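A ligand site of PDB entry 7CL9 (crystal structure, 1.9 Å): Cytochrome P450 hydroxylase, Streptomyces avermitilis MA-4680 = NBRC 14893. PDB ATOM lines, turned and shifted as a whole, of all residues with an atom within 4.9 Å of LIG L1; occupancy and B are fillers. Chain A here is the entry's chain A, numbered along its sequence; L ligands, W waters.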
ATOM      1  N   LEU A  51      11.852  -6.958  16.033  1.00  0.00           N
ATOM      2  CA  LEU A  51      11.744  -5.514  15.695  1.00  0.00           C
ATOM      3  C   LEU A  51      12.385  -5.229  14.308  1.00  0.00           C
ATOM      4  O   LEU A  51      11.934  -4.278  13.617  1.00  0.00           O
ATOM      5  CB  LEU A  51      12.351  -4.656  16.812  1.00  0.00           C
ATOM      6  CG  LEU A  51      11.467  -4.462  18.045  1.00  0.00           C
ATOM      7  CD1 LEU A  51      12.265  -3.825  19.168  1.00  0.00           C
ATOM      8  CD2 LEU A  51      10.261  -3.604  17.702  1.00  0.00           C
ATOM      9  N   LYS A  58       2.812  -3.803  11.004  1.00  0.00           N
ATOM     10  CA  LYS A  58       1.790  -3.017  11.736  1.00  0.00           C
ATOM     11  C   LYS A  58       0.416  -3.164  11.045  1.00  0.00           C
ATOM     12  O   LYS A  58      -0.578  -2.889  11.688  1.00  0.00           O
ATOM     13  CB  LYS A  58       2.203  -1.544  11.741  1.00  0.00           C
ATOM     14  CG  LYS A  58       3.536  -1.211  12.354  1.00  0.00           C
ATOM     15  CD  LYS A  58       3.653  -1.528  13.806  1.00  0.00           C
ATOM     16  CE  LYS A  58       4.665  -0.691  14.542  1.00  0.00           C
ATOM     17  NZ  LYS A  58       4.156   0.644  14.968  1.00  0.00           N
ATOM     18  N   MET A  87       2.877   7.275   9.839  1.00  0.00           N
ATOM     19  CA  MET A  87       4.191   6.627   9.943  1.00  0.00           C
ATOM     20  C   MET A  87       4.108   5.452  10.925  1.00  0.00           C
ATOM     21  O   MET A  87       4.854   4.492  10.726  1.00  0.00           O
ATOM     22  CB  MET A  87       5.120   7.687  10.474  1.00  0.00           C
ATOM     23  CG  MET A  87       6.476   7.247  10.500  1.00  0.00           C
ATOM     24  SD  MET A  87       7.273   8.775  10.588  1.00  0.00           S
ATOM     25  CE  MET A  87       7.346   8.992  12.347  1.00  0.00           C
ATOM     26  N   LEU A  88       3.260   5.503  11.957  1.00  0.00           N
ATOM     27  CA  LEU A  88       3.205   4.447  13.003  1.00  0.00           C
ATOM     28  C   LEU A  88       2.829   3.116  12.363  1.00  0.00           C
ATOM     29  O   LEU A  88       3.293   2.103  12.831  1.00  0.00           O
ATOM     30  CB  LEU A  88       2.164   4.812  14.047  1.00  0.00           C
ATOM     31  CG  LEU A  88       2.073   3.846  15.211  1.00  0.00           C
ATOM     32  CD1 LEU A  88       3.371   3.877  16.028  1.00  0.00           C
ATOM     33  CD2 LEU A  88       0.889   4.242  16.085  1.00  0.00           C
ATOM     34  N   HIS A  95       7.188   3.205   4.723  1.00  0.00           N
ATOM     35  CA  HIS A  95       7.708   3.634   6.050  1.00  0.00           C
ATOM     36  C   HIS A  95       9.061   4.301   5.869  1.00  0.00           C
ATOM     37  O   HIS A  95       9.303   5.359   6.494  1.00  0.00           O
ATOM     38  CB  HIS A  95       7.786   2.440   6.998  1.00  0.00           C
ATOM     39  CG  HIS A  95       8.133   2.860   8.372  1.00  0.00           C
ATOM     40  ND1 HIS A  95       9.328   2.542   8.943  1.00  0.00           N
ATOM     41  CD2 HIS A  95       7.431   3.588   9.262  1.00  0.00           C
ATOM     42  CE1 HIS A  95       9.359   3.062  10.153  1.00  0.00           C
ATOM     43  NE2 HIS A  95       8.201   3.690  10.379  1.00  0.00           N
ATOM     44  N   ARG A  99      10.269   8.021   7.194  1.00  0.00           N
ATOM     45  CA  ARG A  99      11.360   8.174   8.170  1.00  0.00           C
ATOM     46  C   ARG A  99      12.457   9.051   7.570  1.00  0.00           C
ATOM     47  O   ARG A  99      13.042   9.850   8.321  1.00  0.00           O
ATOM     48  CB  ARG A  99      11.852   6.790   8.620  1.00  0.00           C
ATOM     49  CG  ARG A  99      10.808   6.028   9.429  1.00  0.00           C
ATOM     50  CD  ARG A  99      10.344   6.762  10.677  1.00  0.00           C
ATOM     51  NE  ARG A  99      11.464   7.069  11.541  1.00  0.00           N
ATOM     52  CZ  ARG A  99      11.653   6.549  12.751  1.00  0.00           C
ATOM     53  NH1 ARG A  99      10.717   5.748  13.274  1.00  0.00           N
ATOM     54  NH2 ARG A  99      12.740   6.868  13.451  1.00  0.00           N
ATOM     55  N   LEU A 106      13.395  16.589  12.047  1.00  0.00           N
ATOM     56  CA  LEU A 106      13.734  16.390  13.478  1.00  0.00           C
ATOM     57  C   LEU A 106      15.178  15.845  13.611  1.00  0.00           C
ATOM     58  O   LEU A 106      15.401  14.673  13.944  1.00  0.00           O
ATOM     59  CB  LEU A 106      12.693  15.459  14.098  1.00  0.00           C
ATOM     60  CG  LEU A 106      12.753  15.319  15.614  1.00  0.00           C
ATOM     61  CD1 LEU A 106      12.777  16.672  16.323  1.00  0.00           C
ATOM     62  CD2 LEU A 106      11.612  14.461  16.110  1.00  0.00           C
ATOM     63  N   LEU A 231       1.039  12.728  15.812  1.00  0.00           N
ATOM     64  CA  LEU A 231       1.640  11.461  16.299  1.00  0.00           C
ATOM     65  C   LEU A 231       2.749  11.819  17.307  1.00  0.00           C
ATOM     66  O   LEU A 231       2.801  11.183  18.388  1.00  0.00           O
ATOM     67  CB  LEU A 231       2.189  10.696  15.107  1.00  0.00           C
ATOM     68  CG  LEU A 231       2.778   9.339  15.455  1.00  0.00           C
ATOM     69  CD1 LEU A 231       1.691   8.416  15.951  1.00  0.00           C
ATOM     70  CD2 LEU A 231       3.496   8.768  14.240  1.00  0.00           C
ATOM     71  N   MET A 232       3.535  12.841  17.021  1.00  0.00           N
ATOM     72  CA  MET A 232       4.623  13.271  17.948  1.00  0.00           C
ATOM     73  C   MET A 232       4.115  13.780  19.298  1.00  0.00           C
ATOM     74  O   MET A 232       4.785  13.514  20.322  1.00  0.00           O
ATOM     75  CB  MET A 232       5.468  14.346  17.283  1.00  0.00           C
ATOM     76  CG  MET A 232       6.262  13.747  16.135  1.00  0.00           C
ATOM     77  SD  MET A 232       7.323  15.065  15.400  1.00  0.00           S
ATOM     78  CE  MET A 232       8.248  14.040  14.275  1.00  0.00           C
ATOM     79  N   ALA A 235       2.799  10.510  21.069  1.00  0.00           N
ATOM     80  CA  ALA A 235       3.888   9.572  21.411  1.00  0.00           C
ATOM     81  C   ALA A 235       4.825  10.167  22.472  1.00  0.00           C
ATOM     82  O   ALA A 235       5.378   9.395  23.282  1.00  0.00           O
ATOM     83  CB  ALA A 235       4.636   9.203  20.138  1.00  0.00           C
ATOM     84  N   GLY A 236       4.953  11.497  22.500  1.00  0.00           N
ATOM     85  CA  GLY A 236       6.049  12.238  23.181  1.00  0.00           C
ATOM     86  C   GLY A 236       5.695  12.892  24.514  1.00  0.00           C
ATOM     87  O   GLY A 236       6.658  13.203  25.293  1.00  0.00           O
ATOM     88  N   THR A 239       5.054  10.097  27.902  1.00  0.00           N
ATOM     89  CA  THR A 239       6.296   9.309  27.974  1.00  0.00           C
ATOM     90  C   THR A 239       7.409  10.196  28.554  1.00  0.00           C
ATOM     91  O   THR A 239       8.097   9.740  29.465  1.00  0.00           O
ATOM     92  CB  THR A 239       6.704   8.785  26.594  1.00  0.00           C
ATOM     93  OG1 THR A 239       6.656   9.866  25.652  1.00  0.00           O
ATOM     94  CG2 THR A 239       5.827   7.656  26.114  1.00  0.00           C
ATOM     95  N   THR A 240       7.589  11.428  28.052  1.00  0.00           N
ATOM     96  CA  THR A 240       8.667  12.336  28.538  1.00  0.00           C
ATOM     97  C   THR A 240       8.382  12.698  30.005  1.00  0.00           C
ATOM     98  O   THR A 240       9.314  12.683  30.829  1.00  0.00           O
ATOM     99  CB  THR A 240       8.841  13.565  27.651  1.00  0.00           C
ATOM    100  OG1 THR A 240       9.153  13.119  26.328  1.00  0.00           O
ATOM    101  CG2 THR A 240       9.947  14.463  28.159  1.00  0.00           C
ATOM    102  N   LEU A 243       9.365   9.806  32.205  1.00  0.00           N
ATOM    103  CA  LEU A 243      10.837   9.691  32.309  1.00  0.00           C
ATOM    104  C   LEU A 243      11.368  10.598  33.438  1.00  0.00           C
ATOM    105  O   LEU A 243      12.138  10.109  34.243  1.00  0.00           O
ATOM    106  CB  LEU A 243      11.445  10.064  30.959  1.00  0.00           C
ATOM    107  CG  LEU A 243      12.957  10.223  30.945  1.00  0.00           C
ATOM    108  CD1 LEU A 243      13.659   8.966  31.433  1.00  0.00           C
ATOM    109  CD2 LEU A 243      13.435  10.593  29.551  1.00  0.00           C
ATOM    110  N   LEU A 276      15.494   4.860  31.886  1.00  0.00           N
ATOM    111  CA  LEU A 276      14.902   4.334  30.612  1.00  0.00           C
ATOM    112  C   LEU A 276      14.936   2.799  30.607  1.00  0.00           C
ATOM    113  O   LEU A 276      13.939   2.188  30.274  1.00  0.00           O
ATOM    114  CB  LEU A 276      15.713   4.930  29.468  1.00  0.00           C
ATOM    115  CG  LEU A 276      15.304   6.367  29.093  1.00  0.00           C
ATOM    116  CD1 LEU A 276      16.319   6.982  28.154  1.00  0.00           C
ATOM    117  CD2 LEU A 276      13.910   6.363  28.472  1.00  0.00           C
ATOM    118  N   THR A 280      11.220   2.156  32.199  1.00  0.00           N
ATOM    119  CA  THR A 280      10.743   2.799  30.955  1.00  0.00           C
ATOM    120  C   THR A 280       9.331   3.304  31.211  1.00  0.00           C
ATOM    121  O   THR A 280       8.495   2.636  31.819  1.00  0.00           O
ATOM    122  CB  THR A 280      10.853   1.936  29.705  1.00  0.00           C
ATOM    123  OG1 THR A 280      10.198   2.710  28.690  1.00  0.00           O
ATOM    124  CG2 THR A 280      10.232   0.566  29.852  1.00  0.00           C
ATOM    125  N   PRO A 281       9.027   4.510  30.710  1.00  0.00           N
ATOM    126  CA  PRO A 281       7.657   5.007  30.646  1.00  0.00           C
ATOM    127  C   PRO A 281       6.685   4.124  29.826  1.00  0.00           C
ATOM    128  O   PRO A 281       5.497   4.211  30.077  1.00  0.00           O
ATOM    129  CB  PRO A 281       7.815   6.356  29.954  1.00  0.00           C
ATOM    130  CG  PRO A 281       9.259   6.743  30.149  1.00  0.00           C
ATOM    131  CD  PRO A 281      10.017   5.438  30.110  1.00  0.00           C
ATOM    132  N   THR A 282       7.171   3.318  28.881  1.00  0.00           N
ATOM    133  CA  THR A 282       6.313   2.541  27.949  1.00  0.00           C
ATOM    134  C   THR A 282       6.551   1.054  28.215  1.00  0.00           C
ATOM    135  O   THR A 282       7.593   0.498  27.774  1.00  0.00           O
ATOM    136  CB  THR A 282       6.563   2.911  26.478  1.00  0.00           C
ATOM    137  OG1 THR A 282       6.218   4.290  26.386  1.00  0.00           O
ATOM    138  CG2 THR A 282       5.726   2.125  25.497  1.00  0.00           C
ATOM    139  N   VAL A 285       4.297  -1.981  23.787  1.00  0.00           N
ATOM    140  CA  VAL A 285       3.840  -1.341  22.533  1.00  0.00           C
ATOM    141  C   VAL A 285       3.009  -2.329  21.712  1.00  0.00           C
ATOM    142  O   VAL A 285       3.560  -3.411  21.302  1.00  0.00           O
ATOM    143  CB  VAL A 285       5.027  -0.762  21.744  1.00  0.00           C
ATOM    144  CG1 VAL A 285       4.633  -0.383  20.327  1.00  0.00           C
ATOM    145  CG2 VAL A 285       5.637   0.419  22.492  1.00  0.00           C
ATOM    146  N   ARG A 288       1.963  -5.684  16.460  1.00  0.00           N
ATOM    147  CA  ARG A 288       2.532  -6.253  15.232  1.00  0.00           C
ATOM    148  C   ARG A 288       1.833  -7.569  14.914  1.00  0.00           C
ATOM    149  O   ARG A 288       1.260  -8.191  15.816  1.00  0.00           O
ATOM    150  CB  ARG A 288       4.036  -6.436  15.387  1.00  0.00           C
ATOM    151  CG  ARG A 288       4.830  -5.136  15.284  1.00  0.00           C
ATOM    152  CD  ARG A 288       6.245  -5.254  15.842  1.00  0.00           C
ATOM    153  NE  ARG A 288       6.989  -4.067  15.482  1.00  0.00           N
ATOM    154  CZ  ARG A 288       7.129  -2.974  16.220  1.00  0.00           C
ATOM    155  NH1 ARG A 288       6.560  -2.865  17.423  1.00  0.00           N
ATOM    156  NH2 ARG A 288       7.830  -1.973  15.733  1.00  0.00           N
ATOM    157  N   VAL A 309       5.424  -5.684  22.135  1.00  0.00           N
ATOM    158  CA  VAL A 309       6.815  -5.646  22.630  1.00  0.00           C
ATOM    159  C   VAL A 309       6.787  -5.131  24.061  1.00  0.00           C
ATOM    160  O   VAL A 309       6.256  -4.004  24.293  1.00  0.00           O
ATOM    161  CB  VAL A 309       7.691  -4.794  21.693  1.00  0.00           C
ATOM    162  CG1 VAL A 309       9.128  -4.812  22.187  1.00  0.00           C
ATOM    163  CG2 VAL A 309       7.599  -5.308  20.268  1.00  0.00           C
ATOM    164  N   TYR A 311       8.689  -3.793  26.609  1.00  0.00           N
ATOM    165  CA  TYR A 311       9.896  -2.988  26.879  1.00  0.00           C
ATOM    166  C   TYR A 311      10.153  -2.956  28.387  1.00  0.00           C
ATOM    167  O   TYR A 311      11.341  -3.108  28.762  1.00  0.00           O
ATOM    168  CB  TYR A 311       9.733  -1.582  26.303  1.00  0.00           C
ATOM    169  CG  TYR A 311       9.803  -1.554  24.796  1.00  0.00           C
ATOM    170  CD1 TYR A 311      10.995  -1.758  24.138  1.00  0.00           C
ATOM    171  CD2 TYR A 311       8.661  -1.388  24.036  1.00  0.00           C
ATOM    172  CE1 TYR A 311      11.080  -1.735  22.753  1.00  0.00           C
ATOM    173  CE2 TYR A 311       8.714  -1.393  22.644  1.00  0.00           C
ATOM    174  CZ  TYR A 311       9.927  -1.577  22.004  1.00  0.00           C
ATOM    175  OH  TYR A 311       9.999  -1.579  20.653  1.00  0.00           O
ATOM    176  N   SER A 340      14.820   0.834  25.052  1.00  0.00           N
ATOM    177  CA  SER A 340      13.562   1.457  25.538  1.00  0.00           C
ATOM    178  C   SER A 340      13.007   2.453  24.515  1.00  0.00           C
ATOM    179  O   SER A 340      11.848   2.830  24.685  1.00  0.00           O
ATOM    180  CB  SER A 340      13.721   2.012  26.878  1.00  0.00           C
ATOM    181  OG  SER A 340      13.880   0.929  27.803  1.00  0.00           O
ATOM    182  N   PHE A 341      13.793   2.834  23.491  1.00  0.00           N
ATOM    183  CA  PHE A 341      13.312   3.709  22.376  1.00  0.00           C
ATOM    184  C   PHE A 341      12.949   2.857  21.173  1.00  0.00           C
ATOM    185  O   PHE A 341      12.720   3.417  20.078  1.00  0.00           O
ATOM    186  CB  PHE A 341      14.300   4.848  22.049  1.00  0.00           C
ATOM    187  CG  PHE A 341      14.340   5.950  23.076  1.00  0.00           C
ATOM    188  CD1 PHE A 341      13.235   6.730  23.342  1.00  0.00           C
ATOM    189  CD2 PHE A 341      15.504   6.231  23.784  1.00  0.00           C
ATOM    190  CE1 PHE A 341      13.260   7.750  24.280  1.00  0.00           C
ATOM    191  CE2 PHE A 341      15.553   7.276  24.698  1.00  0.00           C
ATOM    192  CZ  PHE A 341      14.410   7.993  24.992  1.00  0.00           C
ATOM    193  N   GLY A 342      12.894   1.539  21.358  1.00  0.00           N
ATOM    194  CA  GLY A 342      12.683   0.615  20.250  1.00  0.00           C
ATOM    195  C   GLY A 342      13.966   0.284  19.542  1.00  0.00           C
ATOM    196  O   GLY A 342      15.041   0.592  20.020  1.00  0.00           O
ATOM    197  N   PRO A 345      13.517  -0.281  12.084  1.00  0.00           N
ATOM    198  CA  PRO A 345      12.922   0.841  11.355  1.00  0.00           C
ATOM    199  C   PRO A 345      12.030   1.780  12.180  1.00  0.00           C
ATOM    200  O   PRO A 345      12.071   3.016  11.906  1.00  0.00           O
ATOM    201  CB  PRO A 345      12.078   0.151  10.259  1.00  0.00           C
ATOM    202  CG  PRO A 345      12.738  -1.195  10.071  1.00  0.00           C
ATOM    203  CD  PRO A 345      13.222  -1.586  11.462  1.00  0.00           C
ATOM    204  N   HIS A 346      11.293   1.255  13.154  1.00  0.00           N
ATOM    205  CA  HIS A 346      10.270   2.045  13.906  1.00  0.00           C
ATOM    206  C   HIS A 346      10.896   2.711  15.121  1.00  0.00           C
ATOM    207  O   HIS A 346      10.145   3.298  15.918  1.00  0.00           O
ATOM    208  CB  HIS A 346       9.027   1.219  14.263  1.00  0.00           C
ATOM    209  CG  HIS A 346       8.105   0.986  13.121  1.00  0.00           C
ATOM    210  ND1 HIS A 346       7.045   1.830  12.854  1.00  0.00           N
ATOM    211  CD2 HIS A 346       8.087   0.042  12.152  1.00  0.00           C
ATOM    212  CE1 HIS A 346       6.409   1.433  11.742  1.00  0.00           C
ATOM    213  NE2 HIS A 346       7.040   0.316  11.289  1.00  0.00           N
ATOM    214  N   VAL A 347      12.223   2.664  15.252  1.00  0.00           N
ATOM    215  CA  VAL A 347      12.920   3.306  16.412  1.00  0.00           C
ATOM    216  C   VAL A 347      12.395   4.732  16.683  1.00  0.00           C
ATOM    217  O   VAL A 347      12.087   5.508  15.777  1.00  0.00           O
ATOM    218  CB  VAL A 347      14.448   3.238  16.238  1.00  0.00           C
ATOM    219  CG1 VAL A 347      14.961   4.134  15.155  1.00  0.00           C
ATOM    220  CG2 VAL A 347      15.166   3.515  17.561  1.00  0.00           C
ATOM    221  N   CYS A 348      12.229   5.093  17.931  1.00  0.00           N
ATOM    222  CA  CYS A 348      11.699   6.415  18.327  1.00  0.00           C
ATOM    223  C   CYS A 348      12.479   7.547  17.662  1.00  0.00           C
ATOM    224  O   CYS A 348      13.679   7.705  17.943  1.00  0.00           O
ATOM    225  CB  CYS A 348      11.800   6.602  19.818  1.00  0.00           C
ATOM    226  SG  CYS A 348      11.076   8.166  20.367  1.00  0.00           S
ATOM    227  N   PRO A 349      11.835   8.420  16.866  1.00  0.00           N
ATOM    228  CA  PRO A 349      12.485   9.611  16.321  1.00  0.00           C
ATOM    229  C   PRO A 349      12.638  10.740  17.327  1.00  0.00           C
ATOM    230  O   PRO A 349      13.355  11.653  17.015  1.00  0.00           O
ATOM    231  CB  PRO A 349      11.541  10.029  15.177  1.00  0.00           C
ATOM    232  CG  PRO A 349      10.188   9.609  15.676  1.00  0.00           C
ATOM    233  CD  PRO A 349      10.444   8.283  16.385  1.00  0.00           C
ATOM    234  N   GLY A 350      11.984  10.661  18.503  1.00  0.00           N
ATOM    235  CA  GLY A 350      12.035  11.684  19.553  1.00  0.00           C
ATOM    236  C   GLY A 350      13.084  11.398  20.630  1.00  0.00           C
ATOM    237  O   GLY A 350      13.125  12.146  21.586  1.00  0.00           O
ATOM    238  N   LEU A 353      15.216  14.255  21.777  1.00  0.00           N
ATOM    239  CA  LEU A 353      14.444  15.329  22.414  1.00  0.00           C
ATOM    240  C   LEU A 353      14.094  14.952  23.842  1.00  0.00           C
ATOM    241  O   LEU A 353      14.238  15.811  24.725  1.00  0.00           O
ATOM    242  CB  LEU A 353      13.184  15.608  21.585  1.00  0.00           C
ATOM    243  CG  LEU A 353      12.309  16.731  22.142  1.00  0.00           C
ATOM    244  CD1 LEU A 353      13.052  18.059  22.135  1.00  0.00           C
ATOM    245  CD2 LEU A 353      11.024  16.842  21.326  1.00  0.00           C
ATOM    246  N   SER A 354      13.575  13.747  24.089  1.00  0.00           N
ATOM    247  CA  SER A 354      13.173  13.327  25.462  1.00  0.00           C
ATOM    248  C   SER A 354      14.437  13.240  26.365  1.00  0.00           C
ATOM    249  O   SER A 354      14.384  13.686  27.493  1.00  0.00           O
ATOM    250  CB  SER A 354      12.348  12.059  25.407  1.00  0.00           C
ATOM    251  OG  SER A 354      13.111  11.025  24.835  1.00  0.00           O
HETATM  252  C1  LIG L   1       7.979   5.392  18.639  1.00  0.00           C
HETATM  253  C2  LIG L   1       9.432   5.294  23.246  1.00  0.00           C
HETATM  254  C3  LIG L   1       9.396  10.118  23.424  1.00  0.00           C
HETATM  255  C4  LIG L   1       7.775  10.186  18.918  1.00  0.00           C
HETATM  256  C5  LIG L   1       8.485   4.942  19.837  1.00  0.00           C
HETATM  257  C6  LIG L   1       8.846   3.598  20.116  1.00  0.00           C
HETATM  258  C7  LIG L   1       9.237   3.579  21.422  1.00  0.00           C
HETATM  259  C8  LIG L   1       9.115   4.900  21.940  1.00  0.00           C
HETATM  260  C9  LIG L   1       9.710   2.325  22.136  1.00  0.00           C
HETATM  261  C10 LIG L   1       8.844   2.397  19.204  1.00  0.00           C
HETATM  262  C11 LIG L   1       7.714   1.456  19.470  1.00  0.00           C
HETATM  263  C12 LIG L   1       7.907   0.225  18.618  1.00  0.00           C
HETATM  264  O1  LIG L   1       7.885  -0.915  19.162  1.00  0.00           O
HETATM  265  O2  LIG L   1       8.062   0.302  17.378  1.00  0.00           O
HETATM  266  C13 LIG L   1       9.471   6.603  23.719  1.00  0.00           C
HETATM  267  C14 LIG L   1       9.897   6.991  25.059  1.00  0.00           C
HETATM  268  C15 LIG L   1       9.845   8.345  25.130  1.00  0.00           C
HETATM  269  C16 LIG L   1       9.465   8.791  23.774  1.00  0.00           C
HETATM  270  C17 LIG L   1      10.171   6.046  26.179  1.00  0.00           C
HETATM  271  C18 LIG L   1      10.189   9.283  26.208  1.00  0.00           C
HETATM  272  C19 LIG L   1      10.942   8.916  27.229  1.00  0.00           C
HETATM  273  C20 LIG L   1       8.972  10.577  22.197  1.00  0.00           C
HETATM  274  C21 LIG L   1       9.057  11.897  21.760  1.00  0.00           C
HETATM  275  C22 LIG L   1       8.594  11.904  20.464  1.00  0.00           C
HETATM  276  C23 LIG L   1       8.266  10.570  20.129  1.00  0.00           C
HETATM  277  C24 LIG L   1       9.553  13.095  22.624  1.00  0.00           C
HETATM  278  C25 LIG L   1       8.468  12.969  19.432  1.00  0.00           C
HETATM  279  C26 LIG L   1       9.004  14.138  19.453  1.00  0.00           C
HETATM  280  C27 LIG L   1       7.681   8.853  18.527  1.00  0.00           C
HETATM  281  C28 LIG L   1       7.106   8.506  17.238  1.00  0.00           C
HETATM  282  C29 LIG L   1       7.160   7.171  17.155  1.00  0.00           C
HETATM  283  C30 LIG L   1       7.767   6.738  18.403  1.00  0.00           C
HETATM  284  C31 LIG L   1       6.579   9.478  16.209  1.00  0.00           C
HETATM  285  C32 LIG L   1       6.721   6.274  16.018  1.00  0.00           C
HETATM  286  C33 LIG L   1       7.895   5.875  15.114  1.00  0.00           C
HETATM  287  C34 LIG L   1       7.517   4.885  14.001  1.00  0.00           C
HETATM  288  O3  LIG L   1       6.636   3.978  14.167  1.00  0.00           O
HETATM  289  O4  LIG L   1       8.090   4.970  12.882  1.00  0.00           O
HETATM  290  N1  LIG L   1       8.677   5.759  20.959  1.00  0.00           N
HETATM  291  N2  LIG L   1       9.327   7.711  22.983  1.00  0.00           N
HETATM  292  N3  LIG L   1       8.556   9.765  21.179  1.00  0.00           N
HETATM  293  N4  LIG L   1       8.011   7.793  19.231  1.00  0.00           N
HETATM  294 FE1  LIG L   1       8.847   7.770  20.952  1.00  0.00          FE
HETATM  295  C1  LG2 L   2       4.130   5.127  20.669  1.00  0.00           C
HETATM  296  C2  LG2 L   2       2.718   4.864  21.246  1.00  0.00           C
HETATM  297  C3  LG2 L   2       1.661   6.116  19.235  1.00  0.00           C
HETATM  298  C4  LG2 L   2       0.560   7.062  18.720  1.00  0.00           C
HETATM  299  C5  LG2 L   2      -0.796   6.769  19.333  1.00  0.00           C
HETATM  300  C6  LG2 L   2      -0.666   6.856  20.859  1.00  0.00           C
HETATM  301  C7  LG2 L   2      -2.117   6.911  21.360  1.00  0.00           C
HETATM  302  C8  LG2 L   2      -2.821   7.794  20.298  1.00  0.00           C
HETATM  303  C9  LG2 L   2      -1.889   7.813  19.097  1.00  0.00           C
HETATM  304  C10 LG2 L   2      -1.417   5.445  18.796  1.00  0.00           C
HETATM  305  C11 LG2 L   2       2.247   3.459  20.806  1.00  0.00           C
HETATM  306  C12 LG2 L   2       5.242   4.420  21.454  1.00  0.00           C
HETATM  307  C13 LG2 L   2       5.206   4.758  22.921  1.00  0.00           C
HETATM  308  C14 LG2 L   2       3.883   4.922  23.490  1.00  0.00           C
HETATM  309  C15 LG2 L   2       2.743   4.901  22.777  1.00  0.00           C
HETATM  310  C16 LG2 L   2       1.409   4.893  23.482  1.00  0.00           C
HETATM  311  C17 LG2 L   2       0.437   5.924  22.938  1.00  0.00           C
HETATM  312  C18 LG2 L   2       0.327   5.836  21.422  1.00  0.00           C
HETATM  313  C19 LG2 L   2       1.731   5.987  20.770  1.00  0.00           C
HETATM  314  O1  LG2 L   2       6.220   4.918  23.601  1.00  0.00           O
HETATM  315  O2  LG2 L   2      -1.999   8.531  18.124  1.00  0.00           O
HETATM  316  O   HOH W   1      11.089   0.043  17.219  1.00  0.00           O
HETATM  317  O   HOH W   2       6.263   1.965  16.290  1.00  0.00           O
HETATM  318  O   HOH W   3       6.538   7.377  22.101  1.00  0.00           O
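SG of Cys 348 binds FE1 of LIG L1 (2.3 Å). An oxygen (O3) of LIG L1 sits at hydrogen-bond distance from a ring nitrogen (ND1) of His 346, 2.6 Å away. The side-chain hydroxyl of Tyr 311 is in hydrogen-bond range of an oxygen (O1) of LIG L1, 2.7 Å away. NH1 of Arg 99 lies within salt-bridge range of O4 of LIG L1 (2.8 Å). NE2 of His 95 is in hydrogen-bond range of O4 of LIG L1, at 2.8 Å. The guanidinium group (NH2) of Arg 288 is in salt-bridge range of an oxygen (O2) of LIG L1 (2.8 Å). OG1 of Thr 282 lies within hydrogen-bond range of O1 of LG2 L2 (2.9 Å).
Water W3 lies within hydrogen-bond range of O of Ala 235 (2.6 Å) and O1 of LG2 L2 (2.9 Å). Water W2 lies within hydrogen-bond range of an oxygen (O2) of LIG L1 (2.7 Å) and the side-chain amino group (NZ) of Lys 58 (2.8 Å). Water W1 lies within hydrogen-bond range of an oxygen (O2) of LIG L1 (3.0 Å) and the backbone NH (N) of Val 347 (3.5 Å).
The backbone NH (N) of Gly 350 sits close to the side-chain sulfur (SG) of Cys 348 (3.2 Å). NE2 of His 95 sits close to ND1 of His 346, at 3.3 Å. NH2 of Arg 99 lies within hydrogen-bond range of O of Val 347, at 2.8 Å. NH1 of Arg 99 lies within hydrogen-bond range of O of Pro 345. The backbone carbonyl oxygen (O) of Gly 236 sits at hydrogen-bond distance from the side-chain hydroxyl (OG1) of Thr 239 (3.4 Å). The backbone carbonyl oxygen (O) of Gly 236 is in hydrogen-bond range of the side-chain hydroxyl (OG1) of Thr 240. OG of Ser 340 sits at hydrogen-bond distance from O of Leu 276. OG1 of Thr 239 is in hydrogen-bond range of O of Ala 235, 2.7 Å away.
Leu 51 touches LIG L1. Met 87 touches LIG L1 (CG to O4, 3.7 Å). Leu 88 touches LIG L1 (CA to O3, 3.7 Å). CD2 of Leu 231 touches C31 of LIG L1, 3.7 Å away. O of Met 232 touches C25 of LIG L1, at 3.8 Å. Ala 235 touches LIG L1. Gly 236 touches LIG L1. Thr 239 touches LIG L1 (CB to C15, 3.5 Å). OG1 of Thr 240 touches C24 of LIG L1, 3.7 Å away. CD2 of Leu 243 touches C19 of LIG L1 (3.8 Å). Pro 281 touches LIG L1 (CD to C17, 3.98 Å). CG1 of Val 285 touches O1 of LIG L1 (3.5 Å). Ser 340 touches LIG L1. C of Phe 341 touches C9 of LIG L1, 3.4 Å away. Gly 342 touches LIG L1 (N to C9, 3.4 Å). Pro 349 touches LIG L1 (CD to C28, 3.5 Å). Gly 350 touches LIG L1 (CA to C22, 3.6 Å). Leu 353 touches LIG L1 (CD2 to C26, 3.9 Å). Ser 354 touches LIG L1. Hydrophobic or aromatic side chains within 4 Å of LIG L1: Leu 51, Met 87, Leu 88, His 95, Leu 231, Met 232, Ala 235, Leu 243, Pro 281, Val 285, Tyr 311, Phe 341, His 346, Pro 349 and Leu 353. Within 4 Å of LIG L1: Leu 51, Met 87, Leu 88, His 95, Arg 99, Leu 231, Met 232, Ala 235, Gly 236, Thr 239, Thr 240, Leu 243, Pro 281, Val 285, Arg 288, Tyr 311, Ser 340, Phe 341, Gly 342, His 346, Cys 348, Pro 349, Gly 350, Leu 353 and Ser 354.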
